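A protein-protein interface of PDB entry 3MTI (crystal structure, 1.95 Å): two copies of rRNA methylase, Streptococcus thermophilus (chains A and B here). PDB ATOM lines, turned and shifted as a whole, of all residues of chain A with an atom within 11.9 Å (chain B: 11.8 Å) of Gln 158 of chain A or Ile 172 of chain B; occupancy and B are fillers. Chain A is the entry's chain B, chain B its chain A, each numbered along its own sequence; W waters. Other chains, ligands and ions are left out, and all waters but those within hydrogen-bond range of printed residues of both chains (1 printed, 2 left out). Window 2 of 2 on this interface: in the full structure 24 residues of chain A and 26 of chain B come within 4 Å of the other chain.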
ATOM      1  N   LEU A 122       4.506   4.220  16.301  1.00  0.00           N
ATOM      2  CA  LEU A 122       5.844   4.764  16.503  1.00  0.00           C
ATOM      3  C   LEU A 122       6.200   5.769  15.409  1.00  0.00           C
ATOM      4  O   LEU A 122       6.701   6.864  15.705  1.00  0.00           O
ATOM      5  CB  LEU A 122       6.883   3.630  16.569  1.00  0.00           C
ATOM      6  CG  LEU A 122       6.856   2.672  17.761  1.00  0.00           C
ATOM      7  CD1 LEU A 122       7.949   1.628  17.635  1.00  0.00           C
ATOM      8  CD2 LEU A 122       6.978   3.429  19.091  1.00  0.00           C
ATOM      9  N   VAL A 127       7.909  13.772  18.706  1.00  0.00           N
ATOM     10  CA  VAL A 127       9.118  13.648  19.510  1.00  0.00           C
ATOM     11  C   VAL A 127       8.683  14.016  20.929  1.00  0.00           C
ATOM     12  O   VAL A 127       7.944  14.976  21.107  1.00  0.00           O
ATOM     13  CB  VAL A 127      10.259  14.568  18.981  1.00  0.00           C
ATOM     14  CG1 VAL A 127      11.467  14.524  19.903  1.00  0.00           C
ATOM     15  CG2 VAL A 127      10.666  14.140  17.577  1.00  0.00           C
ATOM     16  N   LEU A 150       8.231  -7.943  22.407  1.00  0.00           N
ATOM     17  CA  LEU A 150       9.520  -7.753  23.053  1.00  0.00           C
ATOM     18  C   LEU A 150      10.647  -7.802  22.040  1.00  0.00           C
ATOM     19  O   LEU A 150      11.519  -6.945  22.065  1.00  0.00           O
ATOM     20  CB  LEU A 150       9.762  -8.751  24.206  1.00  0.00           C
ATOM     21  CG  LEU A 150       8.955  -8.606  25.506  1.00  0.00           C
ATOM     22  CD1 LEU A 150       9.360  -9.668  26.524  1.00  0.00           C
ATOM     23  CD2 LEU A 150       9.097  -7.201  26.107  1.00  0.00           C
ATOM     24  N   GLU A 151      10.616  -8.784  21.139  1.00  0.00           N
ATOM     25  CA  GLU A 151      11.659  -8.916  20.118  1.00  0.00           C
ATOM     26  C   GLU A 151      11.748  -7.652  19.273  1.00  0.00           C
ATOM     27  O   GLU A 151      12.836  -7.147  18.997  1.00  0.00           O
ATOM     28  CB  GLU A 151      11.436 -10.171  19.243  1.00  0.00           C
ATOM     29  N   TYR A 152      10.596  -7.116  18.898  1.00  0.00           N
ATOM     30  CA  TYR A 152      10.538  -5.895  18.123  1.00  0.00           C
ATOM     31  C   TYR A 152      11.098  -4.678  18.900  1.00  0.00           C
ATOM     32  O   TYR A 152      11.890  -3.913  18.367  1.00  0.00           O
ATOM     33  CB  TYR A 152       9.099  -5.648  17.675  1.00  0.00           C
ATOM     34  CG  TYR A 152       8.937  -4.388  16.886  1.00  0.00           C
ATOM     35  CD1 TYR A 152       8.393  -3.239  17.469  1.00  0.00           C
ATOM     36  CD2 TYR A 152       9.355  -4.327  15.559  1.00  0.00           C
ATOM     37  CE1 TYR A 152       8.250  -2.075  16.730  1.00  0.00           C
ATOM     38  CE2 TYR A 152       9.243  -3.164  14.824  1.00  0.00           C
ATOM     39  CZ  TYR A 152       8.692  -2.049  15.407  1.00  0.00           C
ATOM     40  OH  TYR A 152       8.574  -0.909  14.661  1.00  0.00           O
ATOM     41  N   VAL A 153      10.702  -4.533  20.158  1.00  0.00           N
ATOM     42  CA  VAL A 153      11.104  -3.382  20.981  1.00  0.00           C
ATOM     43  C   VAL A 153      12.610  -3.412  21.245  1.00  0.00           C
ATOM     44  O   VAL A 153      13.292  -2.396  21.092  1.00  0.00           O
ATOM     45  CB  VAL A 153      10.290  -3.326  22.306  1.00  0.00           C
ATOM     46  CG1 VAL A 153      10.774  -2.191  23.209  1.00  0.00           C
ATOM     47  CG2 VAL A 153       8.815  -3.139  21.997  1.00  0.00           C
ATOM     48  N   ILE A 154      13.118  -4.583  21.634  1.00  0.00           N
ATOM     49  CA  ILE A 154      14.560  -4.822  21.812  1.00  0.00           C
ATOM     50  C   ILE A 154      15.367  -4.353  20.574  1.00  0.00           C
ATOM     51  O   ILE A 154      16.380  -3.654  20.703  1.00  0.00           O
ATOM     52  CB  ILE A 154      14.843  -6.319  22.195  1.00  0.00           C
ATOM     53  CG1 ILE A 154      14.254  -6.635  23.580  1.00  0.00           C
ATOM     54  CG2 ILE A 154      16.346  -6.662  22.125  1.00  0.00           C
ATOM     55  CD1 ILE A 154      14.453  -8.052  24.076  1.00  0.00           C
ATOM     56  N   GLY A 155      14.878  -4.703  19.382  1.00  0.00           N
ATOM     57  CA  GLY A 155      15.504  -4.292  18.128  1.00  0.00           C
ATOM     58  C   GLY A 155      15.418  -2.830  17.710  1.00  0.00           C
ATOM     59  O   GLY A 155      16.032  -2.439  16.711  1.00  0.00           O
ATOM     60  N   LEU A 156      14.659  -2.011  18.435  1.00  0.00           N
ATOM     61  CA  LEU A 156      14.597  -0.582  18.110  1.00  0.00           C
ATOM     62  C   LEU A 156      15.924   0.121  18.419  1.00  0.00           C
ATOM     63  O   LEU A 156      16.603  -0.228  19.375  1.00  0.00           O
ATOM     64  CB  LEU A 156      13.443   0.103  18.843  1.00  0.00           C
ATOM     65  CG  LEU A 156      12.003  -0.290  18.494  1.00  0.00           C
ATOM     66  CD1 LEU A 156      11.081   0.233  19.576  1.00  0.00           C
ATOM     67  CD2 LEU A 156      11.590   0.266  17.124  1.00  0.00           C
ATOM     68  N   ASP A 157      16.260   1.102  17.584  1.00  0.00           N
ATOM     69  CA  ASP A 157      17.488   1.891  17.663  1.00  0.00           C
ATOM     70  C   ASP A 157      17.427   2.789  18.888  1.00  0.00           C
ATOM     71  O   ASP A 157      16.610   3.700  18.950  1.00  0.00           O
ATOM     72  CB  ASP A 157      17.575   2.757  16.396  1.00  0.00           C
ATOM     73  CG  ASP A 157      18.907   3.478  16.235  1.00  0.00           C
ATOM     74  OD1 ASP A 157      19.653   3.711  17.223  1.00  0.00           O
ATOM     75  OD2 ASP A 157      19.190   3.846  15.076  1.00  0.00           O
ATOM     76  N   GLN A 158      18.303   2.527  19.852  1.00  0.00           N
ATOM     77  CA  GLN A 158      18.351   3.298  21.111  1.00  0.00           C
ATOM     78  C   GLN A 158      18.538   4.803  20.935  1.00  0.00           C
ATOM     79  O   GLN A 158      18.358   5.571  21.885  1.00  0.00           O
ATOM     80  CB  GLN A 158      19.442   2.744  22.035  1.00  0.00           C
ATOM     81  CG  GLN A 158      20.863   2.869  21.474  1.00  0.00           C
ATOM     82  CD  GLN A 158      21.841   1.993  22.214  1.00  0.00           C
ATOM     83  OE1 GLN A 158      22.566   2.447  23.117  1.00  0.00           O
ATOM     84  NE2 GLN A 158      21.850   0.725  21.870  1.00  0.00           N
ATOM     85  N   ARG A 159      18.921   5.229  19.737  1.00  0.00           N
ATOM     86  CA  ARG A 159      19.162   6.650  19.489  1.00  0.00           C
ATOM     87  C   ARG A 159      17.863   7.312  19.092  1.00  0.00           C
ATOM     88  O   ARG A 159      17.722   8.515  19.212  1.00  0.00           O
ATOM     89  CB  ARG A 159      20.243   6.860  18.424  1.00  0.00           C
ATOM     90  CG  ARG A 159      21.561   6.172  18.802  1.00  0.00           C
ATOM     91  CD  ARG A 159      22.684   6.352  17.783  1.00  0.00           C
ATOM     92  NE  ARG A 159      22.315   6.044  16.405  1.00  0.00           N
ATOM     93  CZ  ARG A 159      22.367   4.842  15.838  1.00  0.00           C
ATOM     94  NH1 ARG A 159      22.756   3.767  16.519  1.00  0.00           N
ATOM     95  NH2 ARG A 159      22.016   4.716  14.569  1.00  0.00           N
ATOM     96  N   VAL A 160      16.905   6.497  18.653  1.00  0.00           N
ATOM     97  CA  VAL A 160      15.611   6.986  18.223  1.00  0.00           C
ATOM     98  C   VAL A 160      14.555   6.769  19.320  1.00  0.00           C
ATOM     99  O   VAL A 160      13.654   7.585  19.505  1.00  0.00           O
ATOM    100  CB  VAL A 160      15.181   6.310  16.866  1.00  0.00           C
ATOM    101  CG1 VAL A 160      13.908   6.921  16.340  1.00  0.00           C
ATOM    102  CG2 VAL A 160      16.299   6.456  15.816  1.00  0.00           C
ATOM    103  N   PHE A 161      14.669   5.663  20.043  1.00  0.00           N
ATOM    104  CA  PHE A 161      13.693   5.307  21.074  1.00  0.00           C
ATOM    105  C   PHE A 161      14.379   4.854  22.356  1.00  0.00           C
ATOM    106  O   PHE A 161      15.465   4.257  22.327  1.00  0.00           O
ATOM    107  CB  PHE A 161      12.773   4.176  20.591  1.00  0.00           C
ATOM    108  CG  PHE A 161      11.849   4.568  19.466  1.00  0.00           C
ATOM    109  CD1 PHE A 161      10.705   5.321  19.716  1.00  0.00           C
ATOM    110  CD2 PHE A 161      12.116   4.170  18.155  1.00  0.00           C
ATOM    111  CE1 PHE A 161       9.848   5.696  18.686  1.00  0.00           C
ATOM    112  CE2 PHE A 161      11.256   4.530  17.100  1.00  0.00           C
ATOM    113  CZ  PHE A 161      10.114   5.286  17.371  1.00  0.00           C
ATOM    114  N   THR A 162      13.745   5.159  23.479  1.00  0.00           N
ATOM    115  CA  THR A 162      14.057   4.515  24.748  1.00  0.00           C
ATOM    116  C   THR A 162      12.926   3.585  25.100  1.00  0.00           C
ATOM    117  O   THR A 162      11.762   3.976  25.088  1.00  0.00           O
ATOM    118  CB  THR A 162      14.331   5.540  25.852  1.00  0.00           C
ATOM    119  OG1 THR A 162      15.482   6.282  25.466  1.00  0.00           O
ATOM    120  CG2 THR A 162      14.640   4.853  27.203  1.00  0.00           C
ATOM    121  N   ALA A 163      13.270   2.328  25.351  1.00  0.00           N
ATOM    122  CA  ALA A 163      12.288   1.322  25.720  1.00  0.00           C
ATOM    123  C   ALA A 163      12.619   0.702  27.076  1.00  0.00           C
ATOM    124  O   ALA A 163      13.746   0.246  27.299  1.00  0.00           O
ATOM    125  CB  ALA A 163      12.200   0.254  24.644  1.00  0.00           C
ATOM    126  N   MET A 164      11.629   0.668  27.965  1.00  0.00           N
ATOM    127  CA  MET A 164      11.821   0.171  29.319  1.00  0.00           C
ATOM    128  C   MET A 164      10.830  -0.935  29.657  1.00  0.00           C
ATOM    129  O   MET A 164       9.653  -0.889  29.263  1.00  0.00           O
ATOM    130  CB  MET A 164      11.641   1.297  30.350  1.00  0.00           C
ATOM    131  CG  MET A 164      12.523   2.520  30.165  1.00  0.00           C
ATOM    132  SD  MET A 164      14.423   2.232  30.598  1.00  0.00           S
ATOM    133  CE  MET A 164      14.305   1.248  32.244  1.00  0.00           C
ATOM    134  N   MET A 180       7.384   0.527  28.204  1.00  0.00           N
ATOM    135  CA  MET A 180       7.313   1.979  28.082  1.00  0.00           C
ATOM    136  C   MET A 180       8.215   2.434  26.939  1.00  0.00           C
ATOM    137  O   MET A 180       9.414   2.167  26.965  1.00  0.00           O
ATOM    138  CB  MET A 180       7.767   2.625  29.398  1.00  0.00           C
ATOM    139  CG  MET A 180       6.784   2.391  30.554  1.00  0.00           C
ATOM    140  SD  MET A 180       7.635   2.338  32.297  1.00  0.00           S
ATOM    141  CE  MET A 180       8.114   4.221  32.524  1.00  0.00           C
ATOM    142  N   LEU A 181       7.651   3.124  25.952  1.00  0.00           N
ATOM    143  CA  LEU A 181       8.419   3.613  24.801  1.00  0.00           C
ATOM    144  C   LEU A 181       8.336   5.128  24.718  1.00  0.00           C
ATOM    145  O   LEU A 181       7.258   5.690  24.840  1.00  0.00           O
ATOM    146  CB  LEU A 181       7.884   2.999  23.491  1.00  0.00           C
ATOM    147  CG  LEU A 181       8.148   1.498  23.306  1.00  0.00           C
ATOM    148  CD1 LEU A 181       7.085   0.820  22.462  1.00  0.00           C
ATOM    149  CD2 LEU A 181       9.465   1.297  22.680  1.00  0.00           C
ATOM    150  N   GLU A 182       9.466   5.800  24.506  1.00  0.00           N
ATOM    151  CA  GLU A 182       9.424   7.230  24.208  1.00  0.00           C
ATOM    152  C   GLU A 182      10.228   7.534  22.952  1.00  0.00           C
ATOM    153  O   GLU A 182      11.284   6.928  22.740  1.00  0.00           O
ATOM    154  CB  GLU A 182       9.956   8.030  25.396  1.00  0.00           C
ATOM    155  CG  GLU A 182       9.874   9.521  25.202  1.00  0.00           C
ATOM    156  CD  GLU A 182      10.258  10.277  26.452  1.00  0.00           C
ATOM    157  OE1 GLU A 182       9.558  10.131  27.470  1.00  0.00           O
ATOM    158  OE2 GLU A 182      11.255  11.016  26.406  1.00  0.00           O
ATOM    159  N   LYS A 183       9.725   8.442  22.114  1.00  0.00           N
ATOM    160  CA  LYS A 183      10.447   8.870  20.920  1.00  0.00           C
ATOM    161  C   LYS A 183      11.436   9.966  21.275  1.00  0.00           C
ATOM    162  O   LYS A 183      11.047  10.962  21.871  1.00  0.00           O
ATOM    163  CB  LYS A 183       9.506   9.401  19.843  1.00  0.00           C
ATOM    164  CG  LYS A 183      10.234   9.720  18.517  1.00  0.00           C
ATOM    165  CD  LYS A 183       9.291  10.089  17.391  1.00  0.00           C
ATOM    166  CE  LYS A 183       8.879   8.874  16.583  1.00  0.00           C
ATOM    167  NZ  LYS A 183       7.983   9.254  15.434  1.00  0.00           N
ATOM    168  N   LEU A 184      12.687   9.781  20.852  1.00  0.00           N
ATOM    169  CA  LEU A 184      13.770  10.746  21.103  1.00  0.00           C
ATOM    170  C   LEU A 184      13.994  11.767  19.968  1.00  0.00           C
ATOM    171  O   LEU A 184      14.431  12.890  20.228  1.00  0.00           O
ATOM    172  CB  LEU A 184      15.074  10.007  21.416  1.00  0.00           C
ATOM    173  CG  LEU A 184      15.035   8.963  22.531  1.00  0.00           C
ATOM    174  CD1 LEU A 184      16.410   8.360  22.736  1.00  0.00           C
ATOM    175  CD2 LEU A 184      14.496   9.577  23.822  1.00  0.00           C
ATOM    176  N   GLN A 185      13.730  11.375  18.722  1.00  0.00           N
ATOM    177  CA  GLN A 185      13.843  12.286  17.544  1.00  0.00           C
ATOM    178  C   GLN A 185      13.144  11.759  16.283  1.00  0.00           C
ATOM    179  O   GLN A 185      12.587  10.661  16.301  1.00  0.00           O
ATOM    180  CB  GLN A 185      15.293  12.729  17.219  1.00  0.00           C
ATOM    181  CG  GLN A 185      16.447  11.885  17.774  1.00  0.00           C
ATOM    182  CD  GLN A 185      16.983  10.858  16.795  1.00  0.00           C
ATOM    183  OE1 GLN A 185      18.192  10.644  16.704  1.00  0.00           O
ATOM    184  NE2 GLN A 185      16.078  10.193  16.074  1.00  0.00           N
ATOM    185  N   ILE B   5      11.853  10.327  30.245  1.00  0.00           N
ATOM    186  CA  ILE B   5      11.740   8.892  30.560  1.00  0.00           C
ATOM    187  C   ILE B   5      12.967   8.584  31.440  1.00  0.00           C
ATOM    188  O   ILE B   5      14.088   8.956  31.090  1.00  0.00           O
ATOM    189  CB  ILE B   5      11.636   7.984  29.299  1.00  0.00           C
ATOM    190  CG1 ILE B   5      11.222   6.562  29.685  1.00  0.00           C
ATOM    191  CG2 ILE B   5      12.928   7.967  28.499  1.00  0.00           C
ATOM    192  CD1 ILE B   5      10.665   5.714  28.530  1.00  0.00           C
ATOM    193  N   ARG B   7      16.042   7.040  33.411  1.00  0.00           N
ATOM    194  CA  ARG B   7      17.083   6.052  33.572  1.00  0.00           C
ATOM    195  C   ARG B   7      16.861   5.384  34.933  1.00  0.00           C
ATOM    196  O   ARG B   7      16.297   6.000  35.844  1.00  0.00           O
ATOM    197  CB  ARG B   7      18.485   6.686  33.492  1.00  0.00           C
ATOM    198  CG  ARG B   7      18.858   7.265  32.126  1.00  0.00           C
ATOM    199  CD  ARG B   7      20.377   7.569  32.006  1.00  0.00           C
ATOM    200  NE  ARG B   7      20.903   8.498  33.028  1.00  0.00           N
ATOM    201  CZ  ARG B   7      20.740   9.827  33.023  1.00  0.00           C
ATOM    202  NH1 ARG B   7      20.021  10.428  32.076  1.00  0.00           N
ATOM    203  NH2 ARG B   7      21.278  10.571  33.993  1.00  0.00           N
ATOM    204  N   GLN B 167      13.915  -2.026  33.848  1.00  0.00           N
ATOM    205  CA  GLN B 167      15.080  -2.463  33.067  1.00  0.00           C
ATOM    206  C   GLN B 167      15.037  -1.919  31.639  1.00  0.00           C
ATOM    207  O   GLN B 167      13.992  -1.956  31.011  1.00  0.00           O
ATOM    208  CB  GLN B 167      15.120  -4.002  33.048  1.00  0.00           C
ATOM    209  CG  GLN B 167      16.273  -4.630  32.260  1.00  0.00           C
ATOM    210  CD  GLN B 167      16.321  -6.131  32.425  1.00  0.00           C
ATOM    211  OE1 GLN B 167      15.409  -6.840  32.010  1.00  0.00           O
ATOM    212  NE2 GLN B 167      17.390  -6.629  33.064  1.00  0.00           N
ATOM    213  N   PRO B 168      16.171  -1.410  31.120  1.00  0.00           N
ATOM    214  CA  PRO B 168      16.163  -0.984  29.725  1.00  0.00           C
ATOM    215  C   PRO B 168      16.099  -2.177  28.762  1.00  0.00           C
ATOM    216  O   PRO B 168      16.683  -3.228  29.031  1.00  0.00           O
ATOM    217  CB  PRO B 168      17.490  -0.237  29.580  1.00  0.00           C
ATOM    218  CG  PRO B 168      17.852   0.171  30.965  1.00  0.00           C
ATOM    219  CD  PRO B 168      17.418  -0.990  31.798  1.00  0.00           C
ATOM    220  N   LEU B 169      15.382  -2.013  27.660  1.00  0.00           N
ATOM    221  CA  LEU B 169      15.184  -3.128  26.718  1.00  0.00           C
ATOM    222  C   LEU B 169      16.093  -3.070  25.504  1.00  0.00           C
ATOM    223  O   LEU B 169      16.697  -4.074  25.133  1.00  0.00           O
ATOM    224  CB  LEU B 169      13.727  -3.192  26.266  1.00  0.00           C
ATOM    225  CG  LEU B 169      12.743  -3.759  27.285  1.00  0.00           C
ATOM    226  CD1 LEU B 169      11.318  -3.538  26.804  1.00  0.00           C
ATOM    227  CD2 LEU B 169      13.040  -5.269  27.566  1.00  0.00           C
ATOM    228  N   ASN B 170      16.211  -1.895  24.914  1.00  0.00           N
ATOM    229  CA  ASN B 170      16.777  -1.733  23.574  1.00  0.00           C
ATOM    230  C   ASN B 170      18.178  -1.109  23.540  1.00  0.00           C
ATOM    231  O   ASN B 170      18.596  -0.515  22.534  1.00  0.00           O
ATOM    232  CB  ASN B 170      15.801  -0.934  22.696  1.00  0.00           C
ATOM    233  CG  ASN B 170      15.722   0.538  23.081  1.00  0.00           C
ATOM    234  OD1 ASN B 170      15.614   1.413  22.213  1.00  0.00           O
ATOM    235  ND2 ASN B 170      15.802   0.822  24.362  1.00  0.00           N
ATOM    236  N   GLN B 171      18.899  -1.232  24.641  1.00  0.00           N
ATOM    237  CA  GLN B 171      20.281  -0.770  24.681  1.00  0.00           C
ATOM    238  C   GLN B 171      21.193  -1.943  24.310  1.00  0.00           C
ATOM    239  O   GLN B 171      21.036  -3.052  24.824  1.00  0.00           O
ATOM    240  CB  GLN B 171      20.621  -0.210  26.056  1.00  0.00           C
ATOM    241  CG  GLN B 171      19.642   0.844  26.518  1.00  0.00           C
ATOM    242  CD  GLN B 171      20.193   2.224  26.366  1.00  0.00           C
ATOM    243  OE1 GLN B 171      21.070   2.638  27.137  1.00  0.00           O
ATOM    244  NE2 GLN B 171      19.695   2.959  25.375  1.00  0.00           N
ATOM    245  N   ILE B 172      22.122  -1.683  23.392  1.00  0.00           N
ATOM    246  CA  ILE B 172      23.025  -2.705  22.859  1.00  0.00           C
ATOM    247  C   ILE B 172      24.013  -3.148  23.935  1.00  0.00           C
ATOM    248  O   ILE B 172      24.110  -4.344  24.244  1.00  0.00           O
ATOM    249  CB  ILE B 172      23.760  -2.199  21.589  1.00  0.00           C
ATOM    250  CG1 ILE B 172      22.773  -2.098  20.418  1.00  0.00           C
ATOM    251  CG2 ILE B 172      24.945  -3.110  21.234  1.00  0.00           C
ATOM    252  CD1 ILE B 172      23.211  -1.165  19.305  1.00  0.00           C
ATOM    253  N   ASN B 173      24.741  -2.183  24.499  1.00  0.00           N
ATOM    254  CA  ASN B 173      25.570  -2.438  25.670  1.00  0.00           C
ATOM    255  C   ASN B 173      24.643  -2.723  26.846  1.00  0.00           C
ATOM    256  O   ASN B 173      23.686  -1.965  27.070  1.00  0.00           O
ATOM    257  CB  ASN B 173      26.455  -1.228  25.971  1.00  0.00           C
ATOM    258  N   THR B 174      24.895  -3.812  27.574  1.00  0.00           N
ATOM    259  CA  THR B 174      24.054  -4.186  28.719  1.00  0.00           C
ATOM    260  C   THR B 174      24.160  -3.142  29.848  1.00  0.00           C
ATOM    261  O   THR B 174      25.205  -3.010  30.480  1.00  0.00           O
ATOM    262  CB  THR B 174      24.394  -5.579  29.262  1.00  0.00           C
ATOM    263  OG1 THR B 174      25.799  -5.656  29.505  1.00  0.00           O
ATOM    264  CG2 THR B 174      23.971  -6.681  28.269  1.00  0.00           C
ATOM    265  N   PRO B 175      23.080  -2.380  30.079  1.00  0.00           N
ATOM    266  CA  PRO B 175      23.129  -1.290  31.048  1.00  0.00           C
ATOM    267  C   PRO B 175      22.652  -1.725  32.450  1.00  0.00           C
ATOM    268  O   PRO B 175      22.159  -2.835  32.613  1.00  0.00           O
ATOM    269  CB  PRO B 175      22.174  -0.260  30.437  1.00  0.00           C
ATOM    270  CG  PRO B 175      21.140  -1.112  29.705  1.00  0.00           C
ATOM    271  CD  PRO B 175      21.758  -2.468  29.428  1.00  0.00           C
ATOM    272  N   PRO B 176      22.812  -0.857  33.459  1.00  0.00           N
ATOM    273  CA  PRO B 176      22.266  -1.171  34.773  1.00  0.00           C
ATOM    274  C   PRO B 176      20.736  -1.251  34.749  1.00  0.00           C
ATOM    275  O   PRO B 176      20.092  -0.588  33.933  1.00  0.00           O
ATOM    276  CB  PRO B 176      22.696   0.028  35.621  1.00  0.00           C
ATOM    277  CG  PRO B 176      23.806   0.675  34.841  1.00  0.00           C
ATOM    278  CD  PRO B 176      23.478   0.457  33.436  1.00  0.00           C
HETATM  279  O   HOH W   1      17.730   5.261  24.500  1.00  0.00           O
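N of Leu 169 of chain B sits at hydrogen-bond distance from O of Ala 163 of chain A (2.8 Å). The side-chain amide oxygen of Asn 170 of chain B lies close to the backbone carbonyl oxygen of Leu 156 of chain A (3.4 Å). O of Phe 161 of chain A lies close to OD1 of Asn 170 of chain B, at 2.9 Å. ND2 of Asn 170 of chain B sits close to N of Ala 163 of chain A (3.1 Å). The backbone NH of Ile 172 of chain B sits close to the side-chain amide nitrogen of Gln 158 of chain A (2.9 Å).
The backbone carbonyl oxygen (O) of Thr 162 of chain A is in hydrogen-bond range of the backbone NH (N) of Glu 182 of chain A, at 3.0 Å. The backbone NH (N) of Met 164 of chain A lies within hydrogen-bond range of the backbone carbonyl oxygen (O) of Met 180 of chain A, 2.9 Å away.
Among the printed residues, merely in contact across the chains: Met 164 of chain A with Gln 167 of chain B (3.3 Å), Val 153 of chain A with Asn 170 of chain B (3.3 Å), Gln 158 of chain A with Gln 171 of chain B (3.4 Å), Gln 158 of chain A with Asn 170 of chain B (3.4 Å), Ile 154 of chain A with Asn 170 of chain B (3.4 Å), Met 164 of chain A with Pro 168 of chain B (3.4 Å), Glu 182 of chain A with Ile 5 of chain B (3.5 Å), Ala 163 of chain A with Pro 168 of chain B (3.6 Å), Thr 162 of chain A with Ile 5 of chain B (3.8 Å), Ile 154 of chain A with Leu 169 of chain B (3.9 Å), Val 153 of chain A with Leu 169 of chain B (3.9 Å) and Met 164 of chain A with Leu 169 of chain B (3.9 Å).
Of chain B, only Asn 170, Gln 171 and Ile 172 come within 4 Å of Gln 158 of chain A. Ile 172 of chain B touches just one residue of chain A: Gln 158 (2.9 Å). Of chain B, only Asn 170 comes within 4 Å of Leu 156 of chain A. No residue of chain B comes within 4 Å of Asp 157 of chain A. Val 160 of chain A touches none of the printed residues of chain B. Thr 162 of chain A touches one residue of chain B. Asn 170 of chain B touches six residues of chain A. Gln 171 of chain B touches just one residue of chain A: Gln 158 (3.4 Å). No residue of chain A comes within 4 Å of Asn 173 of chain B. No residue of chain A comes within 4 Å of Thr 174 of chain B. Printed residues of chain A within 4 Å of Leu 169 of chain B: Val 153, Ile 154, Ala 163 and Met 164. Printed residues of chain B within 4 Å of Met 164 of chain A: Gln 167, Pro 168 and Leu 169. Of the printed residues of chain A, Ile 5 of chain B touches Thr 162 (3.8 Å) and Glu 182 (3.5 Å). Of the printed residues of chain B, Ile 154 of chain A touches Leu 169 and Asn 170. The nearest residue of chain A that does not touch Ile 172 of chain B is Arg 159 of chain A (5.7 Å). The nearest printed residue of chain B that does not touch Met 164 of chain A is Ile 5 of chain B (4.04 Å).
Hydrophobic or aromatic side chains of chain B within 4 Å of the printed part of chain A: Ile 5, Pro 168, Leu 169 and Ile 172.
No position is printed for both chains. Of the 17 pairs that touch across the chains among the printed residues, none has its exchanged pair printed and touching as well.
Water W1 lies within hydrogen-bond range of OG1 of Thr 162 of chain A (2.7 Å), O of Gln 158 of chain A (2.7 Å), NE2 of Gln 171 of chain B (3.2 Å) and O of Phe 161 of chain A (3.3 Å).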
